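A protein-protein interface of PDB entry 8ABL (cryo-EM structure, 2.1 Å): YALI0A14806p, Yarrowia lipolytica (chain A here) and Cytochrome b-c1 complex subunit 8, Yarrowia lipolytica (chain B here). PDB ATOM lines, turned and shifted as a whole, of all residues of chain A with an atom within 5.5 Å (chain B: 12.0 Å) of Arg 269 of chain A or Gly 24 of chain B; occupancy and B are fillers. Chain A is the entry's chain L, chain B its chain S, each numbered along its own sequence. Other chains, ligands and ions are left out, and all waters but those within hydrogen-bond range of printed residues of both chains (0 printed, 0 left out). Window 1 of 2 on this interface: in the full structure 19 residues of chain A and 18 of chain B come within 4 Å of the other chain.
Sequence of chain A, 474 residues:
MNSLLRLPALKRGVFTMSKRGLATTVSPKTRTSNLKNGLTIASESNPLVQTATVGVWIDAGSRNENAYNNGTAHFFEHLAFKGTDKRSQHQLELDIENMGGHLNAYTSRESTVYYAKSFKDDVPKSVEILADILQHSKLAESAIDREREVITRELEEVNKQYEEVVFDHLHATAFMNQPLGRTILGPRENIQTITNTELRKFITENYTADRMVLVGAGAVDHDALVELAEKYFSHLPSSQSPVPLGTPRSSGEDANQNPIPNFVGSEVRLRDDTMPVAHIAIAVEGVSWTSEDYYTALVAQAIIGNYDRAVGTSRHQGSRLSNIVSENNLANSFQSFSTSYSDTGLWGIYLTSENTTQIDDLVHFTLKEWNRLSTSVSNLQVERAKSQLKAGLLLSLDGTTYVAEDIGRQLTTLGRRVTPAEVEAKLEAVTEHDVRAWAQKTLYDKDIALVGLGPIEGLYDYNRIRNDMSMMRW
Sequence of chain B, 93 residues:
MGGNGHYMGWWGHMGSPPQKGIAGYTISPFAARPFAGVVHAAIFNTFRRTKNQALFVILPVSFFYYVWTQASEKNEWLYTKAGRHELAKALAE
O of Thr 26 of chain B lies within hydrogen-bond range of N of Glu 267 of chain A, at 3.0 Å.
O of Gly 24 of chain B sits at hydrogen-bond distance from N of Arg 269 of chain A (2.8 Å).
The side-chain amide nitrogen (NE2) of Gln 19 of chain B sits close to the guanidinium group (NH1) of Arg 271 of chain A, 3.5 Å away.
The guanidinium group of Arg 269 of chain A is in salt-bridge range of the side-chain carboxylate of Glu 267 of chain A (2.8 Å).
The backbone NH (N) of Tyr 462 of chain A lies close to the side-chain carboxylate (OE1) of Glu 267 of chain A (3.2 Å).
The backbone NH of Val 268 of chain A lies within hydrogen-bond range of the backbone carbonyl oxygen of Leu 450 of chain A (2.9 Å).
The backbone NH of Gly 452 of chain A sits at hydrogen-bond distance from the backbone carbonyl oxygen of Val 268 of chain A (3.0 Å).
The guanidinium group of Arg 269 of chain A sits at hydrogen-bond distance from the backbone carbonyl oxygen of Tyr 460 of chain A, 2.9 Å away.
N of Leu 270 of chain A sits at hydrogen-bond distance from O of Gly 452 of chain A (2.7 Å).
Glu 267 of chain A touches Tyr 25 of chain B.
Val 268 of chain A touches Gly 24 of chain B.
CG2 of Val 268 of chain A touches CD2 of Tyr 25 of chain B, at 3.8 Å.
Arg 269 of chain A touches Ile 22 of chain B (O to O, 3.7 Å).
Arg 269 of chain A touches Ala 23 of chain B (O to CA, 3.4 Å).
O of Arg 271 of chain A touches CA of Lys 20 of chain B, at 3.8 Å.
N of Arg 271 of chain A touches O of Ile 22 of chain B, at 3.9 Å.
CE1 of Tyr 460 of chain A touches CE2 of Trp 11 of chain B, 3.7 Å away.
Ser 28 of chain B touches Tyr 462 of chain A (CB to OH, 3.5 Å).
Pro 29 of chain B touches Tyr 462 of chain A.
Arg 269 of chain A touches just these residues of chain B: Ile 22, Ala 23 and Gly 24.
Gly 24 of chain B touches just these residues of chain A: Glu 267, Val 268 and Arg 269.
Of chain B, only Gly 24, Tyr 25 and Thr 26 come within 4 Å of Glu 267 of chain A.
Leu 270 of chain A touches one residue of chain B.
No residue of chain B comes within 4 Å of Gly 452 of chain A.
No residue of chain B comes within 4 Å of Ile 456 of chain A.
No residue of chain B comes within 4 Å of Leu 459 of chain A.
No residue of chain B comes within 4 Å of Asp 461 of chain A.
Printed residues of chain A within 4 Å of Trp 11 of chain B: Tyr 460.
Of the printed residues of chain A, Gln 19 of chain B touches Arg 271 (3.5 Å).
Gly 12 of chain B touches none of the printed residues of chain A.
Ile 27 of chain B touches none of the printed residues of chain A.
Of the 14 printed residues of chain B, 10 touch a printed residue of chain A.
Printed residues of chain B that touch a printed residue of chain A: Trp 11, Gln 19, Lys 20, Ile 22, Ala 23, Gly 24, Tyr 25, Thr 26, Ser 28 and Pro 29.
Of the 12 printed residues of chain A, 7 touch a printed residue of chain B.
Hydrophobic or aromatic side chains of chain A that line the printed part of chain B: Val 268, Leu 270, Tyr 460 and Tyr 462.
Among the printed residues, no Asp or Glu carboxylate lies within 4 Å of a Lys or Arg side-chain nitrogen of the other chain.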
ATOM      1  N   GLU A 267      -2.505   7.618 -21.628  1.00  0.00           N
ATOM      2  CA  GLU A 267      -2.011   6.576 -20.752  1.00  0.00           C
ATOM      3  C   GLU A 267      -0.551   6.826 -20.424  1.00  0.00           C
ATOM      4  O   GLU A 267       0.158   7.472 -21.188  1.00  0.00           O
ATOM      5  CB  GLU A 267      -2.271   5.176 -21.299  1.00  0.00           C
ATOM      6  CG  GLU A 267      -1.920   5.056 -22.747  1.00  0.00           C
ATOM      7  CD  GLU A 267      -1.850   3.621 -23.231  1.00  0.00           C
ATOM      8  OE1 GLU A 267      -2.785   2.834 -22.944  1.00  0.00           O
ATOM      9  OE2 GLU A 267      -0.858   3.287 -23.913  1.00  0.00           O
ATOM     10  N   VAL A 268      -0.153   6.343 -19.250  1.00  0.00           N
ATOM     11  CA  VAL A 268       1.231   6.295 -18.831  1.00  0.00           C
ATOM     12  C   VAL A 268       1.478   4.852 -18.433  1.00  0.00           C
ATOM     13  O   VAL A 268       0.728   4.285 -17.648  1.00  0.00           O
ATOM     14  CB  VAL A 268       1.503   7.242 -17.646  1.00  0.00           C
ATOM     15  CG1 VAL A 268       2.946   7.139 -17.160  1.00  0.00           C
ATOM     16  CG2 VAL A 268       1.145   8.690 -17.962  1.00  0.00           C
ATOM     17  N   ARG A 269       2.512   4.254 -19.009  1.00  0.00           N
ATOM     18  CA  ARG A 269       2.851   2.897 -18.627  1.00  0.00           C
ATOM     19  C   ARG A 269       4.230   2.941 -17.999  1.00  0.00           C
ATOM     20  O   ARG A 269       5.152   3.444 -18.631  1.00  0.00           O
ATOM     21  CB  ARG A 269       2.923   1.997 -19.855  1.00  0.00           C
ATOM     22  CG  ARG A 269       1.568   1.764 -20.499  1.00  0.00           C
ATOM     23  CD  ARG A 269       1.603   1.246 -21.917  1.00  0.00           C
ATOM     24  NE  ARG A 269       0.882   0.015 -21.705  1.00  0.00           N
ATOM     25  CZ  ARG A 269      -0.388  -0.234 -21.972  1.00  0.00           C
ATOM     26  NH1 ARG A 269      -1.178   0.620 -22.598  1.00  0.00           N
ATOM     27  NH2 ARG A 269      -0.837  -1.420 -21.630  1.00  0.00           N
ATOM     28  N   LEU A 270       4.357   2.417 -16.774  1.00  0.00           N
ATOM     29  CA  LEU A 270       5.628   2.416 -16.072  1.00  0.00           C
ATOM     30  C   LEU A 270       5.953   0.965 -15.795  1.00  0.00           C
ATOM     31  O   LEU A 270       5.781   0.474 -14.687  1.00  0.00           O
ATOM     32  CB  LEU A 270       5.488   3.225 -14.778  1.00  0.00           C
ATOM     33  CG  LEU A 270       4.998   4.659 -14.985  1.00  0.00           C
ATOM     34  CD1 LEU A 270       4.393   5.272 -13.722  1.00  0.00           C
ATOM     35  CD2 LEU A 270       6.112   5.538 -15.529  1.00  0.00           C
ATOM     36  N   ARG A 271       6.302   0.255 -16.854  1.00  0.00           N
ATOM     37  CA  ARG A 271       6.447  -1.175 -16.691  1.00  0.00           C
ATOM     38  C   ARG A 271       7.685  -1.479 -15.851  1.00  0.00           C
ATOM     39  O   ARG A 271       8.732  -0.884 -16.065  1.00  0.00           O
ATOM     40  CB  ARG A 271       6.569  -1.836 -18.057  1.00  0.00           C
ATOM     41  CG  ARG A 271       6.859  -3.322 -17.973  1.00  0.00           C
ATOM     42  CD  ARG A 271       6.460  -3.917 -19.303  1.00  0.00           C
ATOM     43  NE  ARG A 271       6.988  -5.265 -19.363  1.00  0.00           N
ATOM     44  CZ  ARG A 271       6.895  -6.078 -20.405  1.00  0.00           C
ATOM     45  NH1 ARG A 271       6.283  -5.687 -21.513  1.00  0.00           N
ATOM     46  NH2 ARG A 271       7.437  -7.281 -20.326  1.00  0.00           N
ATOM     47  N   LEU A 450      -5.267   6.439 -18.003  1.00  0.00           N
ATOM     48  CA  LEU A 450      -4.932   5.107 -17.560  1.00  0.00           C
ATOM     49  C   LEU A 450      -3.481   5.144 -17.111  1.00  0.00           C
ATOM     50  O   LEU A 450      -2.636   5.669 -17.825  1.00  0.00           O
ATOM     51  CB  LEU A 450      -5.136   4.207 -18.783  1.00  0.00           C
ATOM     52  CG  LEU A 450      -4.483   2.832 -18.706  1.00  0.00           C
ATOM     53  CD1 LEU A 450      -5.240   1.949 -17.731  1.00  0.00           C
ATOM     54  CD2 LEU A 450      -4.446   2.170 -20.085  1.00  0.00           C
ATOM     55  N   GLY A 452      -0.489   2.524 -15.586  1.00  0.00           N
ATOM     56  CA  GLY A 452      -0.129   1.224 -15.057  1.00  0.00           C
ATOM     57  C   GLY A 452       1.311   1.223 -14.567  1.00  0.00           C
ATOM     58  O   GLY A 452       2.175   1.790 -15.225  1.00  0.00           O
ATOM     59  N   ILE A 456       3.068  -5.122 -16.115  1.00  0.00           N
ATOM     60  CA  ILE A 456       1.832  -4.783 -16.805  1.00  0.00           C
ATOM     61  C   ILE A 456       1.901  -5.218 -18.269  1.00  0.00           C
ATOM     62  O   ILE A 456       1.163  -4.700 -19.103  1.00  0.00           O
ATOM     63  CB  ILE A 456       1.561  -3.272 -16.665  1.00  0.00           C
ATOM     64  CG1 ILE A 456       2.792  -2.474 -17.119  1.00  0.00           C
ATOM     65  CG2 ILE A 456       1.127  -2.915 -15.243  1.00  0.00           C
ATOM     66  CD1 ILE A 456       2.557  -1.009 -17.433  1.00  0.00           C
ATOM     67  N   LEU A 459      -1.357  -5.782 -19.644  1.00  0.00           N
ATOM     68  CA  LEU A 459      -2.340  -4.721 -19.803  1.00  0.00           C
ATOM     69  C   LEU A 459      -2.403  -4.377 -21.294  1.00  0.00           C
ATOM     70  O   LEU A 459      -1.366  -4.051 -21.842  1.00  0.00           O
ATOM     71  CB  LEU A 459      -1.860  -3.537 -18.954  1.00  0.00           C
ATOM     72  CG  LEU A 459      -2.744  -2.294 -18.989  1.00  0.00           C
ATOM     73  CD1 LEU A 459      -4.118  -2.590 -18.409  1.00  0.00           C
ATOM     74  CD2 LEU A 459      -2.089  -1.154 -18.229  1.00  0.00           C
ATOM     75  N   TYR A 460      -3.557  -4.503 -21.976  1.00  0.00           N
ATOM     76  CA  TYR A 460      -3.591  -4.253 -23.415  1.00  0.00           C
ATOM     77  C   TYR A 460      -3.388  -2.774 -23.725  1.00  0.00           C
ATOM     78  O   TYR A 460      -3.432  -1.939 -22.826  1.00  0.00           O
ATOM     79  CB  TYR A 460      -4.907  -4.723 -24.027  1.00  0.00           C
ATOM     80  CG  TYR A 460      -5.084  -6.221 -24.029  1.00  0.00           C
ATOM     81  CD1 TYR A 460      -4.028  -7.062 -24.354  1.00  0.00           C
ATOM     82  CD2 TYR A 460      -6.303  -6.803 -23.712  1.00  0.00           C
ATOM     83  CE1 TYR A 460      -4.174  -8.441 -24.356  1.00  0.00           C
ATOM     84  CE2 TYR A 460      -6.471  -8.185 -23.718  1.00  0.00           C
ATOM     85  CZ  TYR A 460      -5.395  -9.008 -24.025  1.00  0.00           C
ATOM     86  OH  TYR A 460      -5.505 -10.370 -24.053  1.00  0.00           O
ATOM     87  N   ASP A 461      -3.141  -2.467 -24.996  1.00  0.00           N
ATOM     88  CA  ASP A 461      -2.989  -1.106 -25.485  1.00  0.00           C
ATOM     89  C   ASP A 461      -4.238  -0.265 -25.188  1.00  0.00           C
ATOM     90  O   ASP A 461      -5.308  -0.785 -24.856  1.00  0.00           O
ATOM     91  CB  ASP A 461      -2.675  -1.194 -26.977  1.00  0.00           C
ATOM     92  CG  ASP A 461      -3.624  -2.165 -27.656  1.00  0.00           C
ATOM     93  OD1 ASP A 461      -4.810  -1.832 -27.715  1.00  0.00           O
ATOM     94  OD2 ASP A 461      -3.170  -3.260 -28.113  1.00  0.00           O
ATOM     95  N   TYR A 462      -4.087   1.056 -25.327  1.00  0.00           N
ATOM     96  CA  TYR A 462      -5.143   2.008 -25.032  1.00  0.00           C
ATOM     97  C   TYR A 462      -6.469   1.644 -25.705  1.00  0.00           C
ATOM     98  O   TYR A 462      -7.490   1.690 -25.031  1.00  0.00           O
ATOM     99  CB  TYR A 462      -4.713   3.436 -25.362  1.00  0.00           C
ATOM    100  CG  TYR A 462      -5.678   4.478 -24.852  1.00  0.00           C
ATOM    101  CD1 TYR A 462      -6.749   4.899 -25.630  1.00  0.00           C
ATOM    102  CD2 TYR A 462      -5.554   5.029 -23.580  1.00  0.00           C
ATOM    103  CE1 TYR A 462      -7.660   5.841 -25.164  1.00  0.00           C
ATOM    104  CE2 TYR A 462      -6.464   5.970 -23.100  1.00  0.00           C
ATOM    105  CZ  TYR A 462      -7.511   6.400 -23.901  1.00  0.00           C
ATOM    106  OH  TYR A 462      -8.425   7.321 -23.444  1.00  0.00           O
ATOM    107  N   TRP B  11       0.498 -13.066 -23.497  1.00  0.00           N
ATOM    108  CA  TRP B  11       0.402 -11.870 -22.672  1.00  0.00           C
ATOM    109  C   TRP B  11       0.726 -12.162 -21.205  1.00  0.00           C
ATOM    110  O   TRP B  11       0.178 -13.087 -20.616  1.00  0.00           O
ATOM    111  CB  TRP B  11      -0.991 -11.287 -22.821  1.00  0.00           C
ATOM    112  CG  TRP B  11      -1.289 -10.925 -24.239  1.00  0.00           C
ATOM    113  CD1 TRP B  11      -2.092 -11.609 -25.109  1.00  0.00           C
ATOM    114  CD2 TRP B  11      -0.771  -9.787 -24.959  1.00  0.00           C
ATOM    115  NE1 TRP B  11      -2.130 -10.959 -26.316  1.00  0.00           N
ATOM    116  CE2 TRP B  11      -1.333  -9.837 -26.256  1.00  0.00           C
ATOM    117  CE3 TRP B  11       0.096  -8.725 -24.637  1.00  0.00           C
ATOM    118  CZ2 TRP B  11      -1.048  -8.862 -27.224  1.00  0.00           C
ATOM    119  CZ3 TRP B  11       0.373  -7.759 -25.591  1.00  0.00           C
ATOM    120  CH2 TRP B  11      -0.194  -7.834 -26.870  1.00  0.00           C
ATOM    121  N   GLY B  12       1.631 -11.371 -20.615  1.00  0.00           N
ATOM    122  CA  GLY B  12       2.020 -11.591 -19.233  1.00  0.00           C
ATOM    123  C   GLY B  12       3.318 -12.388 -19.110  1.00  0.00           C
ATOM    124  O   GLY B  12       4.019 -12.247 -18.114  1.00  0.00           O
ATOM    125  N   MET B  14       5.583 -12.906 -22.211  1.00  0.00           N
ATOM    126  CA  MET B  14       5.835 -12.926 -23.644  1.00  0.00           C
ATOM    127  C   MET B  14       7.223 -13.495 -23.960  1.00  0.00           C
ATOM    128  O   MET B  14       7.428 -14.010 -25.055  1.00  0.00           O
ATOM    129  CB  MET B  14       5.669 -11.542 -24.279  1.00  0.00           C
ATOM    130  CG  MET B  14       5.448 -11.581 -25.789  1.00  0.00           C
ATOM    131  SD  MET B  14       3.849 -12.314 -26.239  1.00  0.00           S
ATOM    132  CE  MET B  14       2.734 -11.060 -25.602  1.00  0.00           C
ATOM    133  N   GLN B  19      11.843  -5.795 -18.206  1.00  0.00           N
ATOM    134  CA  GLN B  19      11.838  -4.402 -18.603  1.00  0.00           C
ATOM    135  C   GLN B  19      11.755  -3.542 -17.349  1.00  0.00           C
ATOM    136  O   GLN B  19      11.017  -3.853 -16.416  1.00  0.00           O
ATOM    137  CB  GLN B  19      10.669  -4.113 -19.542  1.00  0.00           C
ATOM    138  CG  GLN B  19      10.621  -5.043 -20.752  1.00  0.00           C
ATOM    139  CD  GLN B  19       9.679  -4.554 -21.830  1.00  0.00           C
ATOM    140  OE1 GLN B  19       9.139  -3.451 -21.761  1.00  0.00           O
ATOM    141  NE2 GLN B  19       9.478  -5.372 -22.851  1.00  0.00           N
ATOM    142  N   LYS B  20      12.526  -2.463 -17.346  1.00  0.00           N
ATOM    143  CA  LYS B  20      12.487  -1.554 -16.225  1.00  0.00           C
ATOM    144  C   LYS B  20      13.040  -0.214 -16.674  1.00  0.00           C
ATOM    145  O   LYS B  20      13.972  -0.173 -17.461  1.00  0.00           O
ATOM    146  CB  LYS B  20      13.369  -2.113 -15.113  1.00  0.00           C
ATOM    147  CG  LYS B  20      13.181  -1.386 -13.805  1.00  0.00           C
ATOM    148  CD  LYS B  20      13.975  -1.992 -12.685  1.00  0.00           C
ATOM    149  CE  LYS B  20      13.773  -1.212 -11.405  1.00  0.00           C
ATOM    150  NZ  LYS B  20      14.536  -1.811 -10.283  1.00  0.00           N
ATOM    151  N   GLY B  21      12.474   0.869 -16.150  1.00  0.00           N
ATOM    152  CA  GLY B  21      13.039   2.186 -16.368  1.00  0.00           C
ATOM    153  C   GLY B  21      12.471   2.893 -17.592  1.00  0.00           C
ATOM    154  O   GLY B  21      12.837   4.033 -17.849  1.00  0.00           O
ATOM    155  N   ILE B  22      11.585   2.242 -18.348  1.00  0.00           N
ATOM    156  CA  ILE B  22      11.032   2.897 -19.529  1.00  0.00           C
ATOM    157  C   ILE B  22       9.638   3.411 -19.187  1.00  0.00           C
ATOM    158  O   ILE B  22       8.809   2.625 -18.761  1.00  0.00           O
ATOM    159  CB  ILE B  22      10.938   1.908 -20.711  1.00  0.00           C
ATOM    160  CG1 ILE B  22      12.282   1.254 -21.049  1.00  0.00           C
ATOM    161  CG2 ILE B  22      10.297   2.578 -21.924  1.00  0.00           C
ATOM    162  CD1 ILE B  22      12.163   0.008 -21.915  1.00  0.00           C
ATOM    163  N   ALA B  23       9.346   4.690 -19.437  1.00  0.00           N
ATOM    164  CA  ALA B  23       7.981   5.154 -19.262  1.00  0.00           C
ATOM    165  C   ALA B  23       7.395   5.386 -20.650  1.00  0.00           C
ATOM    166  O   ALA B  23       8.016   6.084 -21.444  1.00  0.00           O
ATOM    167  CB  ALA B  23       7.995   6.421 -18.438  1.00  0.00           C
ATOM    168  N   GLY B  24       6.224   4.814 -20.953  1.00  0.00           N
ATOM    169  CA  GLY B  24       5.605   5.060 -22.246  1.00  0.00           C
ATOM    170  C   GLY B  24       4.364   5.925 -22.094  1.00  0.00           C
ATOM    171  O   GLY B  24       3.631   5.766 -21.127  1.00  0.00           O
ATOM    172  N   TYR B  25       4.133   6.823 -23.048  1.00  0.00           N
ATOM    173  CA  TYR B  25       3.010   7.736 -22.962  1.00  0.00           C
ATOM    174  C   TYR B  25       2.304   7.719 -24.298  1.00  0.00           C
ATOM    175  O   TYR B  25       2.957   7.588 -25.327  1.00  0.00           O
ATOM    176  CB  TYR B  25       3.512   9.166 -22.763  1.00  0.00           C
ATOM    177  CG  TYR B  25       4.390   9.316 -21.551  1.00  0.00           C
ATOM    178  CD1 TYR B  25       5.729   8.929 -21.571  1.00  0.00           C
ATOM    179  CD2 TYR B  25       3.877   9.835 -20.371  1.00  0.00           C
ATOM    180  CE1 TYR B  25       6.538   9.068 -20.451  1.00  0.00           C
ATOM    181  CE2 TYR B  25       4.668   9.975 -19.241  1.00  0.00           C
ATOM    182  CZ  TYR B  25       5.999   9.594 -19.286  1.00  0.00           C
ATOM    183  OH  TYR B  25       6.764   9.726 -18.169  1.00  0.00           O
ATOM    184  N   THR B  26       0.982   7.864 -24.288  1.00  0.00           N
ATOM    185  CA  THR B  26       0.313   8.131 -25.550  1.00  0.00           C
ATOM    186  C   THR B  26      -1.034   8.773 -25.278  1.00  0.00           C
ATOM    187  O   THR B  26      -1.426   8.867 -24.132  1.00  0.00           O
ATOM    188  CB  THR B  26       0.156   6.860 -26.394  1.00  0.00           C
ATOM    189  OG1 THR B  26      -0.195   7.342 -27.691  1.00  0.00           O
ATOM    190  CG2 THR B  26      -0.902   5.920 -25.865  1.00  0.00           C
ATOM    191  N   ILE B  27      -1.755   9.146 -26.332  1.00  0.00           N
ATOM    192  CA  ILE B  27      -3.023   9.821 -26.134  1.00  0.00           C
ATOM    193  C   ILE B  27      -4.089   9.076 -26.923  1.00  0.00           C
ATOM    194  O   ILE B  27      -3.785   8.379 -27.886  1.00  0.00           O
ATOM    195  CB  ILE B  27      -2.923  11.300 -26.554  1.00  0.00           C
ATOM    196  CG1 ILE B  27      -2.507  11.398 -28.023  1.00  0.00           C
ATOM    197  CG2 ILE B  27      -1.984  12.086 -25.636  1.00  0.00           C
ATOM    198  CD1 ILE B  27      -2.640  12.795 -28.617  1.00  0.00           C
ATOM    199  N   SER B  28      -5.332   9.282 -26.507  1.00  0.00           N
ATOM    200  CA  SER B  28      -6.508   8.642 -27.065  1.00  0.00           C
ATOM    201  C   SER B  28      -6.633   8.940 -28.559  1.00  0.00           C
ATOM    202  O   SER B  28      -6.329  10.048 -28.992  1.00  0.00           O
ATOM    203  CB  SER B  28      -7.698   9.160 -26.318  1.00  0.00           C
ATOM    204  OG  SER B  28      -8.900   8.776 -26.950  1.00  0.00           O
ATOM    205  N   PRO B  29      -7.139   8.004 -29.396  1.00  0.00           N
ATOM    206  CA  PRO B  29      -7.408   8.308 -30.797  1.00  0.00           C
ATOM    207  C   PRO B  29      -8.431   9.429 -30.929  1.00  0.00           C
ATOM    208  O   PRO B  29      -8.374  10.183 -31.886  1.00  0.00           O
ATOM    209  CB  PRO B  29      -8.007   7.022 -31.377  1.00  0.00           C
ATOM    210  CG  PRO B  29      -8.460   6.236 -30.176  1.00  0.00           C
ATOM    211  CD  PRO B  29      -7.512   6.622 -29.058  1.00  0.00           C
